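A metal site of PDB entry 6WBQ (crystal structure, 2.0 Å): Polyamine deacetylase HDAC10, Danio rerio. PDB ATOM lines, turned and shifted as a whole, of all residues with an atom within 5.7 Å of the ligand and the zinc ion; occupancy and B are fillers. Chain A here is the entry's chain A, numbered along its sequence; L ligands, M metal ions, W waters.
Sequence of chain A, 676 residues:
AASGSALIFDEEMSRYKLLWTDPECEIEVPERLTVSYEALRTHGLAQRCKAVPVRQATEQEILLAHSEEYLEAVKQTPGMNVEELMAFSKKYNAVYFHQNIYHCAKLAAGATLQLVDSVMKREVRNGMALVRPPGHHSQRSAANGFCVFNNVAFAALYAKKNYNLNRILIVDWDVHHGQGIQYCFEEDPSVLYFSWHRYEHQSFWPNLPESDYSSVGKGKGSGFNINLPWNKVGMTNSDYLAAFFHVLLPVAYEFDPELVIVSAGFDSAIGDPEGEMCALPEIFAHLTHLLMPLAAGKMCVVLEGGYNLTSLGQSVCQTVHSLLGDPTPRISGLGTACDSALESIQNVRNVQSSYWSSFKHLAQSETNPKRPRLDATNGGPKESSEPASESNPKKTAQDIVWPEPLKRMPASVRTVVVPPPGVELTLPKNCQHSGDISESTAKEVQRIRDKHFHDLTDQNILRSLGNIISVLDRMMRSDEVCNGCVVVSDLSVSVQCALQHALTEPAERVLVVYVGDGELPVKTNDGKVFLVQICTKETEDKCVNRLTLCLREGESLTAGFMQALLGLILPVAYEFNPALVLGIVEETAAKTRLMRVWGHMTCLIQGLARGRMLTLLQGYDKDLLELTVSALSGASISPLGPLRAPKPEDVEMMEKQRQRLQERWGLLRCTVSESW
A nitrogen (N1) of the ligand sits at hydrogen-bond distance from a ring nitrogen (NE2) of His 137, at 2.6 Å.
OH of Tyr 307 sits close to O1 of the ligand.
A ring nitrogen (NE2) of His 136 sits close to an oxygen (O2) of the ligand (2.5 Å).
The indole nitrogen (NE1) of Trp 205 is in hydrogen-bond range of the side-chain amide oxygen (OD1) of Asn 93 (2.7 Å).
The side-chain carboxylate of Asp 267 is in hydrogen-bond range of the backbone NH of Val 175 (2.7 Å).
The backbone NH (N) of His 137 is in hydrogen-bond range of the side-chain sulfur (SG) of Cys 147 (3.5 Å).
OD1 of Asp 22 sits at hydrogen-bond distance from N of Glu 24, 3.1 Å away.
The side-chain carboxylate (OD1) of Asp 174 lies within hydrogen-bond range of the backbone NH (N) of Gly 305 (3.0 Å).
N of Gly 145 is in hydrogen-bond range of O of Asn 93 (3.1 Å).
SG of Cys 147 is in hydrogen-bond range of O of Gly 145 (3.3 Å).
The backbone carbonyl oxygen of Ala 94 sits at hydrogen-bond distance from the backbone NH of Phe 146, 2.8 Å away.
Glu 24 touches the ligand.
SG of Cys 25 touches C20 of the ligand, at 3.98 Å.
Ile 27 touches the ligand.
CB of Ala 94 touches C20 of the ligand, at 3.3 Å.
O of Gly 145 touches C3 of the ligand, at 3.7 Å.
Phe 146 touches the ligand.
CZ of Phe 204 touches C11 of the ligand, 3.8 Å away.
Trp 205 touches the ligand.
Glu 274 touches the ligand.
CA of Gly 305 touches O1 of the ligand, at 3.9996 Å.
Hydrophobic or aromatic side chains that line the ligand: Ile 27, Ala 94, His 136, His 137, Phe 146, His 176, Phe 204, Trp 205 and Tyr 307.
Within 4 Å of the ligand: Glu 24, Cys 25, Ile 27, Ala 94, His 136, His 137, Gly 145, Phe 146, Asp 174, His 176, Phe 204, Trp 205, Asp 267, Glu 274, Gly 305 and Tyr 307.
The nearest printed residue that does not touch the ligand is Asn 93 (4.8 Å).
Three residues have an atom within 4 Å of the zinc ion: Asp 174, His 176 and Asp 267.
The side-chain carboxylate (OD2) of Asp 174 binds the zinc ion, 1.9 Å away.
The side-chain carboxylate (OD2) of Asp 267 is bound to the zinc ion, at 2.1 Å.
The zinc ion is bound by O1 of the ligand (2.1 Å).
O2 of the ligand is bound to the zinc ion (2.1 Å).
The zinc ion is bound by a ring nitrogen (ND1) of His 176 (2.2 Å).
The zinc ion has five donor atoms within binding distance.
Slightly farther from the zinc ion lies the side-chain carboxylate (OD1) of Asp 174 (2.7 Å).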
ATOM      1  N   ASP A  22      18.674 -14.191  23.699  1.00  0.00           N
ATOM      2  CA  ASP A  22      18.044 -15.142  22.795  1.00  0.00           C
ATOM      3  C   ASP A  22      19.140 -16.076  22.323  1.00  0.00           C
ATOM      4  O   ASP A  22      19.898 -15.721  21.397  1.00  0.00           O
ATOM      5  CB  ASP A  22      17.362 -14.427  21.630  1.00  0.00           C
ATOM      6  CG  ASP A  22      16.516 -15.362  20.773  1.00  0.00           C
ATOM      7  OD1 ASP A  22      16.786 -16.590  20.768  1.00  0.00           O
ATOM      8  OD2 ASP A  22      15.595 -14.872  20.099  1.00  0.00           O
ATOM      9  N   GLU A  24      19.163 -18.555  20.440  1.00  0.00           N
ATOM     10  CA  GLU A  24      19.079 -18.949  19.038  1.00  0.00           C
ATOM     11  C   GLU A  24      19.794 -17.952  18.135  1.00  0.00           C
ATOM     12  O   GLU A  24      20.615 -18.340  17.296  1.00  0.00           O
ATOM     13  CB  GLU A  24      17.616 -19.078  18.622  1.00  0.00           C
ATOM     14  CG  GLU A  24      16.810 -20.104  19.385  1.00  0.00           C
ATOM     15  CD  GLU A  24      16.495 -21.328  18.558  1.00  0.00           C
ATOM     16  OE1 GLU A  24      17.283 -21.677  17.648  1.00  0.00           O
ATOM     17  OE2 GLU A  24      15.431 -21.933  18.813  1.00  0.00           O
ATOM     18  N   CYS A  25      19.492 -16.656  18.297  1.00  0.00           N
ATOM     19  CA  CYS A  25      20.028 -15.635  17.403  1.00  0.00           C
ATOM     20  C   CYS A  25      21.407 -15.142  17.797  1.00  0.00           C
ATOM     21  O   CYS A  25      22.017 -14.400  17.018  1.00  0.00           O
ATOM     22  CB  CYS A  25      19.100 -14.408  17.357  1.00  0.00           C
ATOM     23  SG  CYS A  25      17.379 -14.728  16.937  1.00  0.00           S
ATOM     24  N   ILE A  27      24.254 -16.176  17.658  1.00  0.00           N
ATOM     25  CA  ILE A  27      25.406 -16.533  16.846  1.00  0.00           C
ATOM     26  C   ILE A  27      25.651 -15.538  15.732  1.00  0.00           C
ATOM     27  O   ILE A  27      26.730 -15.561  15.126  1.00  0.00           O
ATOM     28  CB  ILE A  27      25.262 -17.937  16.223  1.00  0.00           C
ATOM     29  CG1 ILE A  27      23.972 -18.010  15.402  1.00  0.00           C
ATOM     30  CG2 ILE A  27      25.275 -19.009  17.307  1.00  0.00           C
ATOM     31  CD1 ILE A  27      23.934 -19.215  14.524  1.00  0.00           C
ATOM     32  N   ASN A  93       9.999 -14.666  11.980  1.00  0.00           N
ATOM     33  CA  ASN A  93      10.668 -15.866  12.474  1.00  0.00           C
ATOM     34  C   ASN A  93      12.180 -15.731  12.381  1.00  0.00           C
ATOM     35  O   ASN A  93      12.712 -15.388  11.320  1.00  0.00           O
ATOM     36  CB  ASN A  93      10.178 -17.089  11.683  1.00  0.00           C
ATOM     37  CG  ASN A  93      10.701 -18.396  12.252  1.00  0.00           C
ATOM     38  OD1 ASN A  93      11.308 -19.183  11.541  1.00  0.00           O
ATOM     39  ND2 ASN A  93      10.459 -18.622  13.538  1.00  0.00           N
ATOM     40  N   ALA A  94      12.877 -15.997  13.499  1.00  0.00           N
ATOM     41  CA  ALA A  94      14.329 -16.173  13.539  1.00  0.00           C
ATOM     42  C   ALA A  94      15.080 -14.933  13.045  1.00  0.00           C
ATOM     43  O   ALA A  94      16.074 -15.028  12.320  1.00  0.00           O
ATOM     44  CB  ALA A  94      14.754 -17.422  12.754  1.00  0.00           C
ATOM     45  N   VAL A  95      14.622 -13.758  13.425  1.00  0.00           N
ATOM     46  CA  VAL A  95      15.272 -12.524  13.000  1.00  0.00           C
ATOM     47  C   VAL A  95      15.154 -11.503  14.129  1.00  0.00           C
ATOM     48  O   VAL A  95      14.154 -11.477  14.844  1.00  0.00           O
ATOM     49  CB  VAL A  95      14.681 -12.010  11.671  1.00  0.00           C
ATOM     50  CG1 VAL A  95      13.258 -11.504  11.861  1.00  0.00           C
ATOM     51  CG2 VAL A  95      15.569 -10.905  11.076  1.00  0.00           C
ATOM     52  N   HIS A 136      19.312 -14.494   2.047  1.00  0.00           N
ATOM     53  CA  HIS A 136      18.598 -15.450   1.195  1.00  0.00           C
ATOM     54  C   HIS A 136      17.290 -15.977   1.796  1.00  0.00           C
ATOM     55  O   HIS A 136      16.455 -16.499   1.042  1.00  0.00           O
ATOM     56  CB  HIS A 136      19.534 -16.616   0.760  1.00  0.00           C
ATOM     57  CG  HIS A 136      20.014 -17.505   1.872  1.00  0.00           C
ATOM     58  ND1 HIS A 136      20.394 -18.807   1.661  1.00  0.00           N
ATOM     59  CD2 HIS A 136      20.211 -17.275   3.196  1.00  0.00           C
ATOM     60  CE1 HIS A 136      20.800 -19.347   2.784  1.00  0.00           C
ATOM     61  NE2 HIS A 136      20.707 -18.429   3.736  1.00  0.00           N
ATOM     62  N   HIS A 137      17.054 -15.788   3.088  1.00  0.00           N
ATOM     63  CA  HIS A 137      15.768 -16.133   3.696  1.00  0.00           C
ATOM     64  C   HIS A 137      14.699 -15.048   3.581  1.00  0.00           C
ATOM     65  O   HIS A 137      13.520 -15.356   3.744  1.00  0.00           O
ATOM     66  CB  HIS A 137      15.920 -16.458   5.185  1.00  0.00           C
ATOM     67  CG  HIS A 137      16.779 -17.654   5.450  1.00  0.00           C
ATOM     68  ND1 HIS A 137      16.624 -18.849   4.782  1.00  0.00           N
ATOM     69  CD2 HIS A 137      17.832 -17.825   6.290  1.00  0.00           C
ATOM     70  CE1 HIS A 137      17.541 -19.710   5.209  1.00  0.00           C
ATOM     71  NE2 HIS A 137      18.281 -19.103   6.123  1.00  0.00           N
ATOM     72  N   GLY A 145      15.073 -15.382   9.336  1.00  0.00           N
ATOM     73  CA  GLY A 145      16.356 -16.046   9.463  1.00  0.00           C
ATOM     74  C   GLY A 145      17.556 -15.098   9.375  1.00  0.00           C
ATOM     75  O   GLY A 145      18.440 -15.314   8.545  1.00  0.00           O
ATOM     76  N   PHE A 146      17.575 -14.047  10.201  1.00  0.00           N
ATOM     77  CA  PHE A 146      18.593 -12.990  10.229  1.00  0.00           C
ATOM     78  C   PHE A 146      18.586 -12.102   8.984  1.00  0.00           C
ATOM     79  O   PHE A 146      19.360 -11.139   8.951  1.00  0.00           O
ATOM     80  CB  PHE A 146      20.027 -13.530  10.387  1.00  0.00           C
ATOM     81  CG  PHE A 146      20.237 -14.358  11.600  1.00  0.00           C
ATOM     82  CD1 PHE A 146      19.591 -14.049  12.785  1.00  0.00           C
ATOM     83  CD2 PHE A 146      21.068 -15.462  11.559  1.00  0.00           C
ATOM     84  CE1 PHE A 146      19.779 -14.827  13.903  1.00  0.00           C
ATOM     85  CE2 PHE A 146      21.265 -16.212  12.668  1.00  0.00           C
ATOM     86  CZ  PHE A 146      20.623 -15.899  13.845  1.00  0.00           C
ATOM     87  N   CYS A 147      17.763 -12.384   7.971  1.00  0.00           N
ATOM     88  CA  CYS A 147      17.753 -11.607   6.735  1.00  0.00           C
ATOM     89  C   CYS A 147      16.632 -10.573   6.716  1.00  0.00           C
ATOM     90  O   CYS A 147      15.475 -10.872   7.060  1.00  0.00           O
ATOM     91  CB  CYS A 147      17.628 -12.527   5.512  1.00  0.00           C
ATOM     92  SG  CYS A 147      18.762 -13.906   5.542  1.00  0.00           S
ATOM     93  N   ASP A 174      25.205 -22.090   1.172  1.00  0.00           N
ATOM     94  CA  ASP A 174      24.881 -21.947   2.581  1.00  0.00           C
ATOM     95  C   ASP A 174      24.256 -23.263   3.030  1.00  0.00           C
ATOM     96  O   ASP A 174      23.735 -24.013   2.193  1.00  0.00           O
ATOM     97  CB  ASP A 174      23.910 -20.767   2.791  1.00  0.00           C
ATOM     98  CG  ASP A 174      23.698 -20.407   4.240  1.00  0.00           C
ATOM     99  OD1 ASP A 174      24.324 -19.447   4.731  1.00  0.00           O
ATOM    100  OD2 ASP A 174      22.857 -21.049   4.917  1.00  0.00           O
ATOM    101  N   VAL A 175      24.317 -23.558   4.334  1.00  0.00           N
ATOM    102  CA  VAL A 175      23.786 -24.840   4.795  1.00  0.00           C
ATOM    103  C   VAL A 175      22.284 -24.793   5.020  1.00  0.00           C
ATOM    104  O   VAL A 175      21.667 -25.850   5.241  1.00  0.00           O
ATOM    105  CB  VAL A 175      24.539 -25.287   6.074  1.00  0.00           C
ATOM    106  CG1 VAL A 175      23.929 -24.650   7.313  1.00  0.00           C
ATOM    107  CG2 VAL A 175      24.589 -26.842   6.156  1.00  0.00           C
ATOM    108  N   HIS A 176      21.676 -23.615   4.973  1.00  0.00           N
ATOM    109  CA  HIS A 176      20.237 -23.448   5.090  1.00  0.00           C
ATOM    110  C   HIS A 176      19.630 -23.249   3.711  1.00  0.00           C
ATOM    111  O   HIS A 176      20.283 -22.758   2.784  1.00  0.00           O
ATOM    112  CB  HIS A 176      19.899 -22.239   5.982  1.00  0.00           C
ATOM    113  CG  HIS A 176      20.371 -22.393   7.400  1.00  0.00           C
ATOM    114  ND1 HIS A 176      21.609 -21.978   7.823  1.00  0.00           N
ATOM    115  CD2 HIS A 176      19.765 -22.936   8.481  1.00  0.00           C
ATOM    116  CE1 HIS A 176      21.743 -22.221   9.112  1.00  0.00           C
ATOM    117  NE2 HIS A 176      20.635 -22.810   9.532  1.00  0.00           N
ATOM    118  N   PHE A 204      14.682 -30.016  10.056  1.00  0.00           N
ATOM    119  CA  PHE A 204      15.599 -28.903  10.311  1.00  0.00           C
ATOM    120  C   PHE A 204      15.022 -27.596   9.764  1.00  0.00           C
ATOM    121  O   PHE A 204      14.472 -27.564   8.661  1.00  0.00           O
ATOM    122  CB  PHE A 204      16.995 -29.158   9.719  1.00  0.00           C
ATOM    123  CG  PHE A 204      18.043 -28.223  10.267  1.00  0.00           C
ATOM    124  CD1 PHE A 204      18.370 -28.250  11.612  1.00  0.00           C
ATOM    125  CD2 PHE A 204      18.666 -27.292   9.435  1.00  0.00           C
ATOM    126  CE1 PHE A 204      19.316 -27.366  12.138  1.00  0.00           C
ATOM    127  CE2 PHE A 204      19.625 -26.409   9.954  1.00  0.00           C
ATOM    128  CZ  PHE A 204      19.948 -26.456  11.312  1.00  0.00           C
ATOM    129  N   TRP A 205      15.135 -26.538  10.566  1.00  0.00           N
ATOM    130  CA  TRP A 205      14.702 -25.211  10.168  1.00  0.00           C
ATOM    131  C   TRP A 205      15.187 -24.892   8.753  1.00  0.00           C
ATOM    132  O   TRP A 205      16.337 -25.212   8.408  1.00  0.00           O
ATOM    133  CB  TRP A 205      15.221 -24.179  11.174  1.00  0.00           C
ATOM    134  CG  TRP A 205      14.621 -22.839  11.000  1.00  0.00           C
ATOM    135  CD1 TRP A 205      13.520 -22.342  11.648  1.00  0.00           C
ATOM    136  CD2 TRP A 205      15.063 -21.816  10.099  1.00  0.00           C
ATOM    137  NE1 TRP A 205      13.251 -21.077  11.193  1.00  0.00           N
ATOM    138  CE2 TRP A 205      14.167 -20.729  10.233  1.00  0.00           C
ATOM    139  CE3 TRP A 205      16.118 -21.722   9.188  1.00  0.00           C
ATOM    140  CZ2 TRP A 205      14.306 -19.547   9.507  1.00  0.00           C
ATOM    141  CZ3 TRP A 205      16.257 -20.527   8.443  1.00  0.00           C
ATOM    142  CH2 TRP A 205      15.353 -19.461   8.613  1.00  0.00           C
ATOM    143  N   GLY A 265      27.140 -19.033   1.939  1.00  0.00           N
ATOM    144  CA  GLY A 265      27.127 -19.240   3.365  1.00  0.00           C
ATOM    145  C   GLY A 265      28.160 -20.299   3.701  1.00  0.00           C
ATOM    146  O   GLY A 265      28.203 -21.351   3.059  1.00  0.00           O
ATOM    147  N   ASP A 267      28.367 -21.600   6.717  1.00  0.00           N
ATOM    148  CA  ASP A 267      27.896 -22.501   7.753  1.00  0.00           C
ATOM    149  C   ASP A 267      27.769 -23.935   7.256  1.00  0.00           C
ATOM    150  O   ASP A 267      27.365 -24.808   8.028  1.00  0.00           O
ATOM    151  CB  ASP A 267      26.565 -22.004   8.327  1.00  0.00           C
ATOM    152  CG  ASP A 267      25.545 -21.644   7.264  1.00  0.00           C
ATOM    153  OD1 ASP A 267      25.690 -22.015   6.076  1.00  0.00           O
ATOM    154  OD2 ASP A 267      24.563 -20.986   7.645  1.00  0.00           O
ATOM    155  N   GLU A 274      25.546 -24.438  13.336  1.00  0.00           N
ATOM    156  CA  GLU A 274      24.259 -24.626  12.680  1.00  0.00           C
ATOM    157  C   GLU A 274      24.269 -25.803  11.706  1.00  0.00           C
ATOM    158  O   GLU A 274      23.346 -26.619  11.697  1.00  0.00           O
ATOM    159  CB  GLU A 274      23.849 -23.342  11.941  1.00  0.00           C
ATOM    160  CG  GLU A 274      23.232 -22.310  12.861  1.00  0.00           C
ATOM    161  CD  GLU A 274      21.802 -22.665  13.230  1.00  0.00           C
ATOM    162  OE1 GLU A 274      21.094 -23.229  12.362  1.00  0.00           O
ATOM    163  OE2 GLU A 274      21.393 -22.392  14.381  1.00  0.00           O
ATOM    164  N   GLU A 304      26.548 -15.067   2.893  1.00  0.00           N
ATOM    165  CA  GLU A 304      25.315 -15.315   3.628  1.00  0.00           C
ATOM    166  C   GLU A 304      25.686 -15.615   5.065  1.00  0.00           C
ATOM    167  O   GLU A 304      26.062 -14.688   5.815  1.00  0.00           O
ATOM    168  CB  GLU A 304      24.481 -16.421   2.951  1.00  0.00           C
ATOM    169  CG  GLU A 304      24.064 -16.114   1.520  1.00  0.00           C
ATOM    170  CD  GLU A 304      22.866 -15.149   1.410  1.00  0.00           C
ATOM    171  OE1 GLU A 304      22.379 -14.643   2.436  1.00  0.00           O
ATOM    172  OE2 GLU A 304      22.402 -14.899   0.288  1.00  0.00           O
ATOM    173  N   GLY A 305      25.621 -16.874   5.519  1.00  0.00           N
ATOM    174  CA  GLY A 305      25.940 -17.218   6.888  1.00  0.00           C
ATOM    175  C   GLY A 305      27.349 -17.788   7.068  1.00  0.00           C
ATOM    176  O   GLY A 305      28.220 -17.683   6.206  1.00  0.00           O
ATOM    177  N   GLY A 306      27.548 -18.407   8.237  1.00  0.00           N
ATOM    178  CA  GLY A 306      28.860 -18.887   8.672  1.00  0.00           C
ATOM    179  C   GLY A 306      29.155 -18.361  10.065  1.00  0.00           C
ATOM    180  O   GLY A 306      29.291 -17.146  10.256  1.00  0.00           O
ATOM    181  N   TYR A 307      29.226 -19.242  11.058  1.00  0.00           N
ATOM    182  CA  TYR A 307      29.179 -18.811  12.450  1.00  0.00           C
ATOM    183  C   TYR A 307      30.323 -19.319  13.305  1.00  0.00           C
ATOM    184  O   TYR A 307      30.454 -18.857  14.438  1.00  0.00           O
ATOM    185  CB  TYR A 307      27.833 -19.222  13.084  1.00  0.00           C
ATOM    186  CG  TYR A 307      26.711 -18.717  12.237  1.00  0.00           C
ATOM    187  CD1 TYR A 307      26.337 -17.379  12.277  1.00  0.00           C
ATOM    188  CD2 TYR A 307      26.092 -19.550  11.306  1.00  0.00           C
ATOM    189  CE1 TYR A 307      25.354 -16.893  11.464  1.00  0.00           C
ATOM    190  CE2 TYR A 307      25.117 -19.073  10.482  1.00  0.00           C
ATOM    191  CZ  TYR A 307      24.740 -17.747  10.562  1.00  0.00           C
ATOM    192  OH  TYR A 307      23.761 -17.257   9.741  1.00  0.00           O
HETATM  193  O1  LIG L   1      22.695 -19.045   8.347  1.00  0.00           O
HETATM  194  C1  LIG L   1      21.494 -18.960   8.458  1.00  0.00           C
HETATM  195  N1  LIG L   1      20.662 -18.948   7.236  1.00  0.00           N
HETATM  196  O2  LIG L   1      21.395 -18.997   6.050  1.00  0.00           O
HETATM  197  C2  LIG L   1      20.791 -18.930   9.803  1.00  0.00           C
HETATM  198  C3  LIG L   1      19.468 -18.529   9.935  1.00  0.00           C
HETATM  199  C4  LIG L   1      18.814 -18.534  11.157  1.00  0.00           C
HETATM  200  C5  LIG L   1      19.430 -18.941  12.331  1.00  0.00           C
HETATM  201  C6  LIG L   1      20.758 -19.351  12.209  1.00  0.00           C
HETATM  202  C7  LIG L   1      21.425 -19.349  10.979  1.00  0.00           C
HETATM  203  C8  LIG L   1      18.711 -18.880  13.682  1.00  0.00           C
HETATM  204  N2  LIG L   1      17.632 -19.795  14.091  1.00  0.00           N
HETATM  205  C9  LIG L   1      17.497 -21.140  13.761  1.00  0.00           C
HETATM  206  C10 LIG L   1      18.406 -21.967  12.913  1.00  0.00           C
HETATM  207  C11 LIG L   1      18.149 -23.477  12.917  1.00  0.00           C
HETATM  208  N3  LIG L   1      17.471 -23.878  14.098  1.00  0.00           N
HETATM  209  C12 LIG L   1      18.436 -23.719  15.279  1.00  0.00           C
HETATM  210  C13 LIG L   1      16.081 -23.073  14.196  1.00  0.00           C
HETATM  211  C14 LIG L   1      16.377 -21.643  14.354  1.00  0.00           C
HETATM  212  C15 LIG L   1      15.722 -20.622  15.109  1.00  0.00           C
HETATM  213  C16 LIG L   1      16.522 -19.457  14.939  1.00  0.00           C
HETATM  214  C17 LIG L   1      14.562 -20.556  15.909  1.00  0.00           C
HETATM  215  C18 LIG L   1      14.206 -19.364  16.512  1.00  0.00           C
HETATM  216  C19 LIG L   1      14.998 -18.215  16.331  1.00  0.00           C
HETATM  217  C20 LIG L   1      16.154 -18.256  15.575  1.00  0.00           C
HETATM  218 ZN    ZN M   1      22.790 -20.413   6.758  1.00  0.00          ZN
HETATM  219  O   HOH W   1      15.849 -26.762  13.436  1.00  0.00           O
